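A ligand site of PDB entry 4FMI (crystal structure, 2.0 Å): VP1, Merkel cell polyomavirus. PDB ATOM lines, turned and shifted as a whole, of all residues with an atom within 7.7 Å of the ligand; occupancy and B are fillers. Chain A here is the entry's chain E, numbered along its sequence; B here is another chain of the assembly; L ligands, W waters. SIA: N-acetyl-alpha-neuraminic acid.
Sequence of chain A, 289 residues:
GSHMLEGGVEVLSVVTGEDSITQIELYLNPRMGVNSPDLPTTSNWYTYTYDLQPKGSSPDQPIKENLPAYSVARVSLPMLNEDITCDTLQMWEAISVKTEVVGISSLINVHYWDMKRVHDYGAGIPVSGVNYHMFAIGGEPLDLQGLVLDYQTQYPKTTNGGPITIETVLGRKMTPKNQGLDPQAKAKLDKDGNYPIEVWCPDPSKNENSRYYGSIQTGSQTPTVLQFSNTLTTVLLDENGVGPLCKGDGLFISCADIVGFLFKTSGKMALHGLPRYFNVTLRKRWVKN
N of Lys 268 is in hydrogen-bond range of OG of Ser 266. The side-chain carboxylate of Asp 51 lies within salt-bridge range of the side-chain amino group of Lys 264 (2.8 Å). The backbone carbonyl oxygen of Asp 51 is in hydrogen-bond range of the side-chain amide nitrogen of Asn 66. The backbone NH of Tyr 50 sits at hydrogen-bond distance from the side-chain amide oxygen of Asn 66. O of Glu 65 is in hydrogen-bond range of N of Tyr 50, 3.1 Å away.
The side-chain hydroxyl (OG) of Ser 266 sits at hydrogen-bond distance from an oxygen (O1A) of the ligand (2.5 Å). A nitrogen (N5) of the ligand lies within hydrogen-bond range of the side-chain carboxylate of Asp 51 (2.6 Å). O4 of the ligand is in hydrogen-bond range of NZ of Lys 264, 2.8 Å away. NZ of Lys 268 lies within salt-bridge range of O1B of the ligand (3.6 Å). NE1 of Trp 45 sits at hydrogen-bond distance from O10 of the ligand (3.3 Å).
Residues that only touch the ligand: Tyr 50 (3.6 Å). Hydrophobic or aromatic side chains within 4 Å of the ligand: Trp 45 and Tyr 50. Within 4 Å of the ligand: Trp 45, Tyr 50, Asp 51, Lys 264, Ser 266 and Lys 268. Along chain A the residues within 4 Å of the ligand span positions 45 to 268.
Water W1 lies within hydrogen-bond range of O1A of the ligand (2.6 Å), OD2 of Asp 114 (2.7 Å), N of Ser 266 (3.0 Å) and N of Thr 265 (3.5 Å). Water W3 lies within hydrogen-bond range of an oxygen (O4) of the ligand (2.8 Å), the side-chain hydroxyl of Tyr 112 (2.9 Å) and the side-chain carboxylate of Asp 114 (2.9 Å). Water W2 lies within hydrogen-bond range of OD1 of Asp 51 (2.6 Å), NZ of Lys 268 (2.8 Å) and O9 of the ligand (3.1 Å).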
ATOM      1  N   VAL A  34     -14.772 -21.542  26.346  1.00  0.00           N
ATOM      2  CA  VAL A  34     -14.412 -21.168  27.705  1.00  0.00           C
ATOM      3  C   VAL A  34     -15.744 -20.998  28.399  1.00  0.00           C
ATOM      4  O   VAL A  34     -16.417 -19.966  28.246  1.00  0.00           O
ATOM      5  CB  VAL A  34     -13.573 -19.865  27.764  1.00  0.00           C
ATOM      6  CG1 VAL A  34     -13.160 -19.556  29.195  1.00  0.00           C
ATOM      7  CG2 VAL A  34     -12.353 -19.968  26.867  1.00  0.00           C
ATOM      8  N   TRP A  45     -11.675 -15.200  28.836  1.00  0.00           N
ATOM      9  CA  TRP A  45     -12.309 -15.498  27.564  1.00  0.00           C
ATOM     10  C   TRP A  45     -13.707 -16.155  27.675  1.00  0.00           C
ATOM     11  O   TRP A  45     -14.270 -16.613  26.688  1.00  0.00           O
ATOM     12  CB  TRP A  45     -11.373 -16.303  26.660  1.00  0.00           C
ATOM     13  CG  TRP A  45     -10.262 -15.444  26.143  1.00  0.00           C
ATOM     14  CD1 TRP A  45      -8.913 -15.607  26.369  1.00  0.00           C
ATOM     15  CD2 TRP A  45     -10.382 -14.277  25.335  1.00  0.00           C
ATOM     16  NE1 TRP A  45      -8.199 -14.614  25.737  1.00  0.00           N
ATOM     17  CE2 TRP A  45      -9.074 -13.785  25.090  1.00  0.00           C
ATOM     18  CE3 TRP A  45     -11.477 -13.591  24.772  1.00  0.00           C
ATOM     19  CZ2 TRP A  45      -8.834 -12.639  24.323  1.00  0.00           C
ATOM     20  CZ3 TRP A  45     -11.238 -12.454  24.015  1.00  0.00           C
ATOM     21  CH2 TRP A  45      -9.924 -11.992  23.801  1.00  0.00           C
ATOM     22  N   THR A  49     -14.848 -18.343  22.141  1.00  0.00           N
ATOM     23  CA  THR A  49     -13.927 -19.420  21.806  1.00  0.00           C
ATOM     24  C   THR A  49     -12.499 -18.918  22.001  1.00  0.00           C
ATOM     25  O   THR A  49     -12.283 -17.762  22.394  1.00  0.00           O
ATOM     26  CB  THR A  49     -14.078 -19.892  20.340  1.00  0.00           C
ATOM     27  OG1 THR A  49     -13.842 -18.790  19.445  1.00  0.00           O
ATOM     28  CG2 THR A  49     -15.464 -20.471  20.088  1.00  0.00           C
ATOM     29  N   TYR A  50     -11.546 -19.806  21.730  1.00  0.00           N
ATOM     30  CA  TYR A  50     -10.179 -19.411  21.498  1.00  0.00           C
ATOM     31  C   TYR A  50     -10.084 -19.087  20.007  1.00  0.00           C
ATOM     32  O   TYR A  50     -11.117 -18.905  19.340  1.00  0.00           O
ATOM     33  CB  TYR A  50      -9.239 -20.559  21.865  1.00  0.00           C
ATOM     34  CG  TYR A  50      -8.850 -20.618  23.328  1.00  0.00           C
ATOM     35  CD1 TYR A  50      -9.497 -19.846  24.283  1.00  0.00           C
ATOM     36  CD2 TYR A  50      -7.824 -21.462  23.746  1.00  0.00           C
ATOM     37  CE1 TYR A  50      -9.126 -19.897  25.626  1.00  0.00           C
ATOM     38  CE2 TYR A  50      -7.434 -21.526  25.089  1.00  0.00           C
ATOM     39  CZ  TYR A  50      -8.100 -20.742  26.024  1.00  0.00           C
ATOM     40  OH  TYR A  50      -7.741 -20.803  27.347  1.00  0.00           O
ATOM     41  N   ASP A  51      -8.873 -19.006  19.474  1.00  0.00           N
ATOM     42  CA  ASP A  51      -8.703 -18.556  18.109  1.00  0.00           C
ATOM     43  C   ASP A  51      -8.984 -19.683  17.135  1.00  0.00           C
ATOM     44  O   ASP A  51      -8.398 -20.767  17.210  1.00  0.00           O
ATOM     45  CB  ASP A  51      -7.311 -17.942  17.900  1.00  0.00           C
ATOM     46  CG  ASP A  51      -7.035 -16.775  18.863  1.00  0.00           C
ATOM     47  OD1 ASP A  51      -5.949 -16.764  19.474  1.00  0.00           O
ATOM     48  OD2 ASP A  51      -7.908 -15.891  19.025  1.00  0.00           O
ATOM     49  N   LEU A  52      -9.938 -19.437  16.236  1.00  0.00           N
ATOM     50  CA  LEU A  52     -10.332 -20.420  15.237  1.00  0.00           C
ATOM     51  C   LEU A  52      -9.473 -20.269  14.002  1.00  0.00           C
ATOM     52  O   LEU A  52      -9.414 -19.197  13.407  1.00  0.00           O
ATOM     53  CB  LEU A  52     -11.802 -20.267  14.871  1.00  0.00           C
ATOM     54  CG  LEU A  52     -12.793 -20.679  15.964  1.00  0.00           C
ATOM     55  CD1 LEU A  52     -14.117 -19.962  15.800  1.00  0.00           C
ATOM     56  CD2 LEU A  52     -12.994 -22.205  16.003  1.00  0.00           C
ATOM     57  N   GLN A  53      -8.795 -21.359  13.627  1.00  0.00           N
ATOM     58  CA  GLN A  53      -7.905 -21.370  12.477  1.00  0.00           C
ATOM     59  C   GLN A  53      -7.953 -22.736  11.820  1.00  0.00           C
ATOM     60  O   GLN A  53      -8.046 -23.750  12.513  1.00  0.00           O
ATOM     61  CB  GLN A  53      -6.448 -21.127  12.900  1.00  0.00           C
ATOM     62  CG  GLN A  53      -6.130 -19.783  13.568  1.00  0.00           C
ATOM     63  CD  GLN A  53      -4.657 -19.655  13.894  1.00  0.00           C
ATOM     64  OE1 GLN A  53      -3.842 -19.356  13.025  1.00  0.00           O
ATOM     65  NE2 GLN A  53      -4.291 -19.920  15.144  1.00  0.00           N
ATOM     66  N   ILE A  63      -9.685 -28.223  19.690  1.00  0.00           N
ATOM     67  CA  ILE A  63      -9.688 -28.195  21.159  1.00  0.00           C
ATOM     68  C   ILE A  63     -11.081 -27.862  21.688  1.00  0.00           C
ATOM     69  O   ILE A  63     -11.923 -27.353  20.941  1.00  0.00           O
ATOM     70  CB  ILE A  63      -8.661 -27.161  21.697  1.00  0.00           C
ATOM     71  CG1 ILE A  63      -8.985 -25.749  21.171  1.00  0.00           C
ATOM     72  CG2 ILE A  63      -7.210 -27.587  21.351  1.00  0.00           C
ATOM     73  CD1 ILE A  63      -8.033 -24.668  21.667  1.00  0.00           C
ATOM     74  N   GLU A  65     -12.106 -25.560  23.695  1.00  0.00           N
ATOM     75  CA  GLU A  65     -12.308 -24.124  23.759  1.00  0.00           C
ATOM     76  C   GLU A  65     -12.748 -23.550  22.420  1.00  0.00           C
ATOM     77  O   GLU A  65     -13.205 -22.399  22.362  1.00  0.00           O
ATOM     78  CB  GLU A  65     -11.038 -23.413  24.227  1.00  0.00           C
ATOM     79  CG  GLU A  65     -10.731 -23.573  25.713  1.00  0.00           C
ATOM     80  CD  GLU A  65     -10.011 -24.877  26.045  1.00  0.00           C
ATOM     81  OE1 GLU A  65      -9.688 -25.671  25.101  1.00  0.00           O
ATOM     82  OE2 GLU A  65      -9.763 -25.120  27.244  1.00  0.00           O
ATOM     83  N   ASN A  66     -12.595 -24.337  21.364  1.00  0.00           N
ATOM     84  CA  ASN A  66     -13.057 -23.953  20.031  1.00  0.00           C
ATOM     85  C   ASN A  66     -14.327 -24.653  19.583  1.00  0.00           C
ATOM     86  O   ASN A  66     -14.652 -24.642  18.402  1.00  0.00           O
ATOM     87  CB  ASN A  66     -11.961 -24.176  18.998  1.00  0.00           C
ATOM     88  CG  ASN A  66     -10.889 -23.113  19.055  1.00  0.00           C
ATOM     89  OD1 ASN A  66     -11.096 -22.032  19.630  1.00  0.00           O
ATOM     90  ND2 ASN A  66      -9.733 -23.409  18.475  1.00  0.00           N
ATOM     91  N   TYR A 112     -12.730  -2.360  21.600  1.00  0.00           N
ATOM     92  CA  TYR A 112     -12.021  -3.408  22.344  1.00  0.00           C
ATOM     93  C   TYR A 112     -10.511  -3.161  22.117  1.00  0.00           C
ATOM     94  O   TYR A 112     -10.085  -2.834  20.996  1.00  0.00           O
ATOM     95  CB  TYR A 112     -12.468  -4.810  21.878  1.00  0.00           C
ATOM     96  CG  TYR A 112     -11.547  -5.944  22.305  1.00  0.00           C
ATOM     97  CD1 TYR A 112     -11.402  -6.290  23.657  1.00  0.00           C
ATOM     98  CD2 TYR A 112     -10.790  -6.648  21.358  1.00  0.00           C
ATOM     99  CE1 TYR A 112     -10.540  -7.327  24.061  1.00  0.00           C
ATOM    100  CE2 TYR A 112      -9.927  -7.675  21.752  1.00  0.00           C
ATOM    101  CZ  TYR A 112      -9.811  -8.009  23.093  1.00  0.00           C
ATOM    102  OH  TYR A 112      -8.955  -9.015  23.476  1.00  0.00           O
ATOM    103  N   TRP A 113      -9.702  -3.263  23.171  1.00  0.00           N
ATOM    104  CA  TRP A 113      -8.298  -2.808  23.077  1.00  0.00           C
ATOM    105  C   TRP A 113      -7.518  -3.491  21.959  1.00  0.00           C
ATOM    106  O   TRP A 113      -6.675  -2.855  21.338  1.00  0.00           O
ATOM    107  CB  TRP A 113      -7.559  -2.894  24.411  1.00  0.00           C
ATOM    108  CG  TRP A 113      -7.202  -4.282  24.846  1.00  0.00           C
ATOM    109  CD1 TRP A 113      -7.925  -5.087  25.682  1.00  0.00           C
ATOM    110  CD2 TRP A 113      -6.030  -5.028  24.480  1.00  0.00           C
ATOM    111  NE1 TRP A 113      -7.283  -6.296  25.841  1.00  0.00           N
ATOM    112  CE2 TRP A 113      -6.121  -6.286  25.131  1.00  0.00           C
ATOM    113  CE3 TRP A 113      -4.927  -4.761  23.662  1.00  0.00           C
ATOM    114  CZ2 TRP A 113      -5.140  -7.273  24.983  1.00  0.00           C
ATOM    115  CZ3 TRP A 113      -3.926  -5.751  23.524  1.00  0.00           C
ATOM    116  CH2 TRP A 113      -4.056  -6.994  24.184  1.00  0.00           C
ATOM    117  N   ASP A 114      -7.819  -4.764  21.689  1.00  0.00           N
ATOM    118  CA  ASP A 114      -7.101  -5.536  20.674  1.00  0.00           C
ATOM    119  C   ASP A 114      -7.998  -5.841  19.483  1.00  0.00           C
ATOM    120  O   ASP A 114      -7.921  -6.917  18.877  1.00  0.00           O
ATOM    121  CB  ASP A 114      -6.544  -6.852  21.277  1.00  0.00           C
ATOM    122  CG  ASP A 114      -5.346  -7.393  20.484  1.00  0.00           C
ATOM    123  OD1 ASP A 114      -4.676  -6.607  19.819  1.00  0.00           O
ATOM    124  OD2 ASP A 114      -5.089  -8.621  20.524  1.00  0.00           O
ATOM    125  N   LEU A 262     -15.186 -11.941  17.243  1.00  0.00           N
ATOM    126  CA  LEU A 262     -14.317 -10.880  17.710  1.00  0.00           C
ATOM    127  C   LEU A 262     -13.074 -10.875  16.820  1.00  0.00           C
ATOM    128  O   LEU A 262     -12.313 -11.842  16.821  1.00  0.00           O
ATOM    129  CB  LEU A 262     -13.917 -11.102  19.178  1.00  0.00           C
ATOM    130  CG  LEU A 262     -13.073  -9.994  19.803  1.00  0.00           C
ATOM    131  CD1 LEU A 262     -13.853  -8.669  19.880  1.00  0.00           C
ATOM    132  CD2 LEU A 262     -12.556 -10.424  21.178  1.00  0.00           C
ATOM    133  N   LYS A 264      -9.460  -9.726  16.075  1.00  0.00           N
ATOM    134  CA  LYS A 264      -8.291  -9.266  16.821  1.00  0.00           C
ATOM    135  C   LYS A 264      -7.228  -8.656  15.911  1.00  0.00           C
ATOM    136  O   LYS A 264      -7.169  -8.963  14.711  1.00  0.00           O
ATOM    137  CB  LYS A 264      -7.715 -10.405  17.678  1.00  0.00           C
ATOM    138  CG  LYS A 264      -8.707 -11.001  18.677  1.00  0.00           C
ATOM    139  CD  LYS A 264      -8.180 -12.313  19.310  1.00  0.00           C
ATOM    140  CE  LYS A 264      -9.195 -12.937  20.280  1.00  0.00           C
ATOM    141  NZ  LYS A 264      -8.632 -14.108  21.048  1.00  0.00           N
ATOM    142  N   THR A 265      -6.393  -7.789  16.494  1.00  0.00           N
ATOM    143  CA  THR A 265      -5.344  -7.040  15.770  1.00  0.00           C
ATOM    144  C   THR A 265      -4.499  -7.926  14.839  1.00  0.00           C
ATOM    145  O   THR A 265      -4.271  -7.577  13.677  1.00  0.00           O
ATOM    146  CB  THR A 265      -4.403  -6.284  16.767  1.00  0.00           C
ATOM    147  OG1 THR A 265      -5.189  -5.408  17.589  1.00  0.00           O
ATOM    148  CG2 THR A 265      -3.344  -5.445  16.040  1.00  0.00           C
ATOM    149  N   SER A 266      -4.061  -9.059  15.376  1.00  0.00           N
ATOM    150  CA  SER A 266      -3.151  -9.985  14.685  1.00  0.00           C
ATOM    151  C   SER A 266      -3.748 -10.649  13.446  1.00  0.00           C
ATOM    152  O   SER A 266      -3.019 -11.156  12.602  1.00  0.00           O
ATOM    153  CB  SER A 266      -2.743 -11.091  15.652  1.00  0.00           C
ATOM    154  OG  SER A 266      -3.914 -11.784  16.073  1.00  0.00           O
ATOM    155  N   GLY A 267      -5.079 -10.665  13.376  1.00  0.00           N
ATOM    156  CA  GLY A 267      -5.806 -11.398  12.328  1.00  0.00           C
ATOM    157  C   GLY A 267      -6.645 -12.509  12.914  1.00  0.00           C
ATOM    158  O   GLY A 267      -7.611 -12.948  12.297  1.00  0.00           O
ATOM    159  N   LYS A 268      -6.307 -12.923  14.128  1.00  0.00           N
ATOM    160  CA  LYS A 268      -7.058 -13.971  14.811  1.00  0.00           C
ATOM    161  C   LYS A 268      -8.503 -13.578  15.108  1.00  0.00           C
ATOM    162  O   LYS A 268      -8.844 -12.376  15.209  1.00  0.00           O
ATOM    163  CB  LYS A 268      -6.301 -14.505  16.029  1.00  0.00           C
ATOM    164  CG  LYS A 268      -5.025 -15.226  15.563  1.00  0.00           C
ATOM    165  CD  LYS A 268      -4.188 -15.773  16.662  1.00  0.00           C
ATOM    166  CE  LYS A 268      -3.116 -16.686  16.061  1.00  0.00           C
ATOM    167  NZ  LYS A 268      -2.192 -17.185  17.098  1.00  0.00           N
ATOM    168  N   MET A 269      -9.330 -14.606  15.191  1.00  0.00           N
ATOM    169  CA  MET A 269     -10.775 -14.472  15.276  1.00  0.00           C
ATOM    170  C   MET A 269     -11.314 -15.506  16.229  1.00  0.00           C
ATOM    171  O   MET A 269     -11.013 -16.704  16.098  1.00  0.00           O
ATOM    172  CB  MET A 269     -11.373 -14.727  13.903  1.00  0.00           C
ATOM    173  CG  MET A 269     -11.281 -13.558  12.975  1.00  0.00           C
ATOM    174  SD  MET A 269     -11.362 -14.047  11.260  1.00  0.00           S
ATOM    175  CE  MET A 269     -13.121 -14.369  11.059  1.00  0.00           C
ATOM    176  N   ALA A 270     -12.119 -15.037  17.174  1.00  0.00           N
ATOM    177  CA  ALA A 270     -12.812 -15.923  18.093  1.00  0.00           C
ATOM    178  C   ALA A 270     -14.308 -15.719  17.985  1.00  0.00           C
ATOM    179  O   ALA A 270     -14.778 -14.592  17.779  1.00  0.00           O
ATOM    180  CB  ALA A 270     -12.336 -15.682  19.526  1.00  0.00           C
ATOM    181  N   TYR B 121      -3.942 -15.316   9.503  1.00  0.00           N
ATOM    182  CA  TYR B 121      -4.167 -15.718  10.907  1.00  0.00           C
ATOM    183  C   TYR B 121      -5.643 -15.844  11.270  1.00  0.00           C
ATOM    184  O   TYR B 121      -5.994 -16.128  12.430  1.00  0.00           O
ATOM    185  CB  TYR B 121      -3.419 -14.809  11.879  1.00  0.00           C
ATOM    186  CG  TYR B 121      -1.922 -14.764  11.598  1.00  0.00           C
ATOM    187  CD1 TYR B 121      -1.338 -13.685  10.943  1.00  0.00           C
ATOM    188  CD2 TYR B 121      -1.093 -15.827  11.992  1.00  0.00           C
ATOM    189  CE1 TYR B 121       0.036 -13.655  10.683  1.00  0.00           C
ATOM    190  CE2 TYR B 121       0.270 -15.805  11.732  1.00  0.00           C
ATOM    191  CZ  TYR B 121       0.834 -14.725  11.078  1.00  0.00           C
ATOM    192  OH  TYR B 121       2.186 -14.711  10.838  1.00  0.00           O
HETATM  193  C1  SIA L   1      -2.867 -13.031  19.086  1.00  0.00           C
HETATM  194  C2  SIA L   1      -2.760 -12.925  20.603  1.00  0.00           C
HETATM  195  C3  SIA L   1      -4.074 -12.437  21.227  1.00  0.00           C
HETATM  196  C4  SIA L   1      -5.151 -13.535  21.312  1.00  0.00           C
HETATM  197  C5  SIA L   1      -4.590 -14.811  21.933  1.00  0.00           C
HETATM  198  C6  SIA L   1      -3.301 -15.258  21.238  1.00  0.00           C
HETATM  199  C7  SIA L   1      -2.619 -16.445  21.937  1.00  0.00           C
HETATM  200  C8  SIA L   1      -1.251 -16.818  21.359  1.00  0.00           C
HETATM  201  C9  SIA L   1      -0.891 -18.271  21.686  1.00  0.00           C
HETATM  202  C10 SIA L   1      -6.146 -16.427  22.985  1.00  0.00           C
HETATM  203  C11 SIA L   1      -7.201 -17.440  22.667  1.00  0.00           C
HETATM  204  N5  SIA L   1      -5.618 -15.838  21.916  1.00  0.00           N
HETATM  205  O1A SIA L   1      -3.705 -12.306  18.502  1.00  0.00           O
HETATM  206  O1B SIA L   1      -2.101 -13.817  18.471  1.00  0.00           O
HETATM  207  O2  SIA L   1      -1.733 -11.979  20.923  1.00  0.00           O
HETATM  208  O4  SIA L   1      -6.260 -13.086  22.097  1.00  0.00           O
HETATM  209  O6  SIA L   1      -2.348 -14.185  21.164  1.00  0.00           O
HETATM  210  O7  SIA L   1      -2.444 -16.110  23.317  1.00  0.00           O
HETATM  211  O8  SIA L   1      -1.190 -16.608  19.942  1.00  0.00           O
HETATM  212  O9  SIA L   1      -1.525 -19.153  20.733  1.00  0.00           O
HETATM  213  O10 SIA L   1      -5.818 -16.167  24.137  1.00  0.00           O
HETATM  214  O   HOH W   1      -4.090  -9.708  18.278  1.00  0.00           O
HETATM  215  O   HOH W   2      -3.887 -18.334  18.975  1.00  0.00           O
HETATM  216  O   HOH W   3      -6.701 -10.350  22.219  1.00  0.00           O
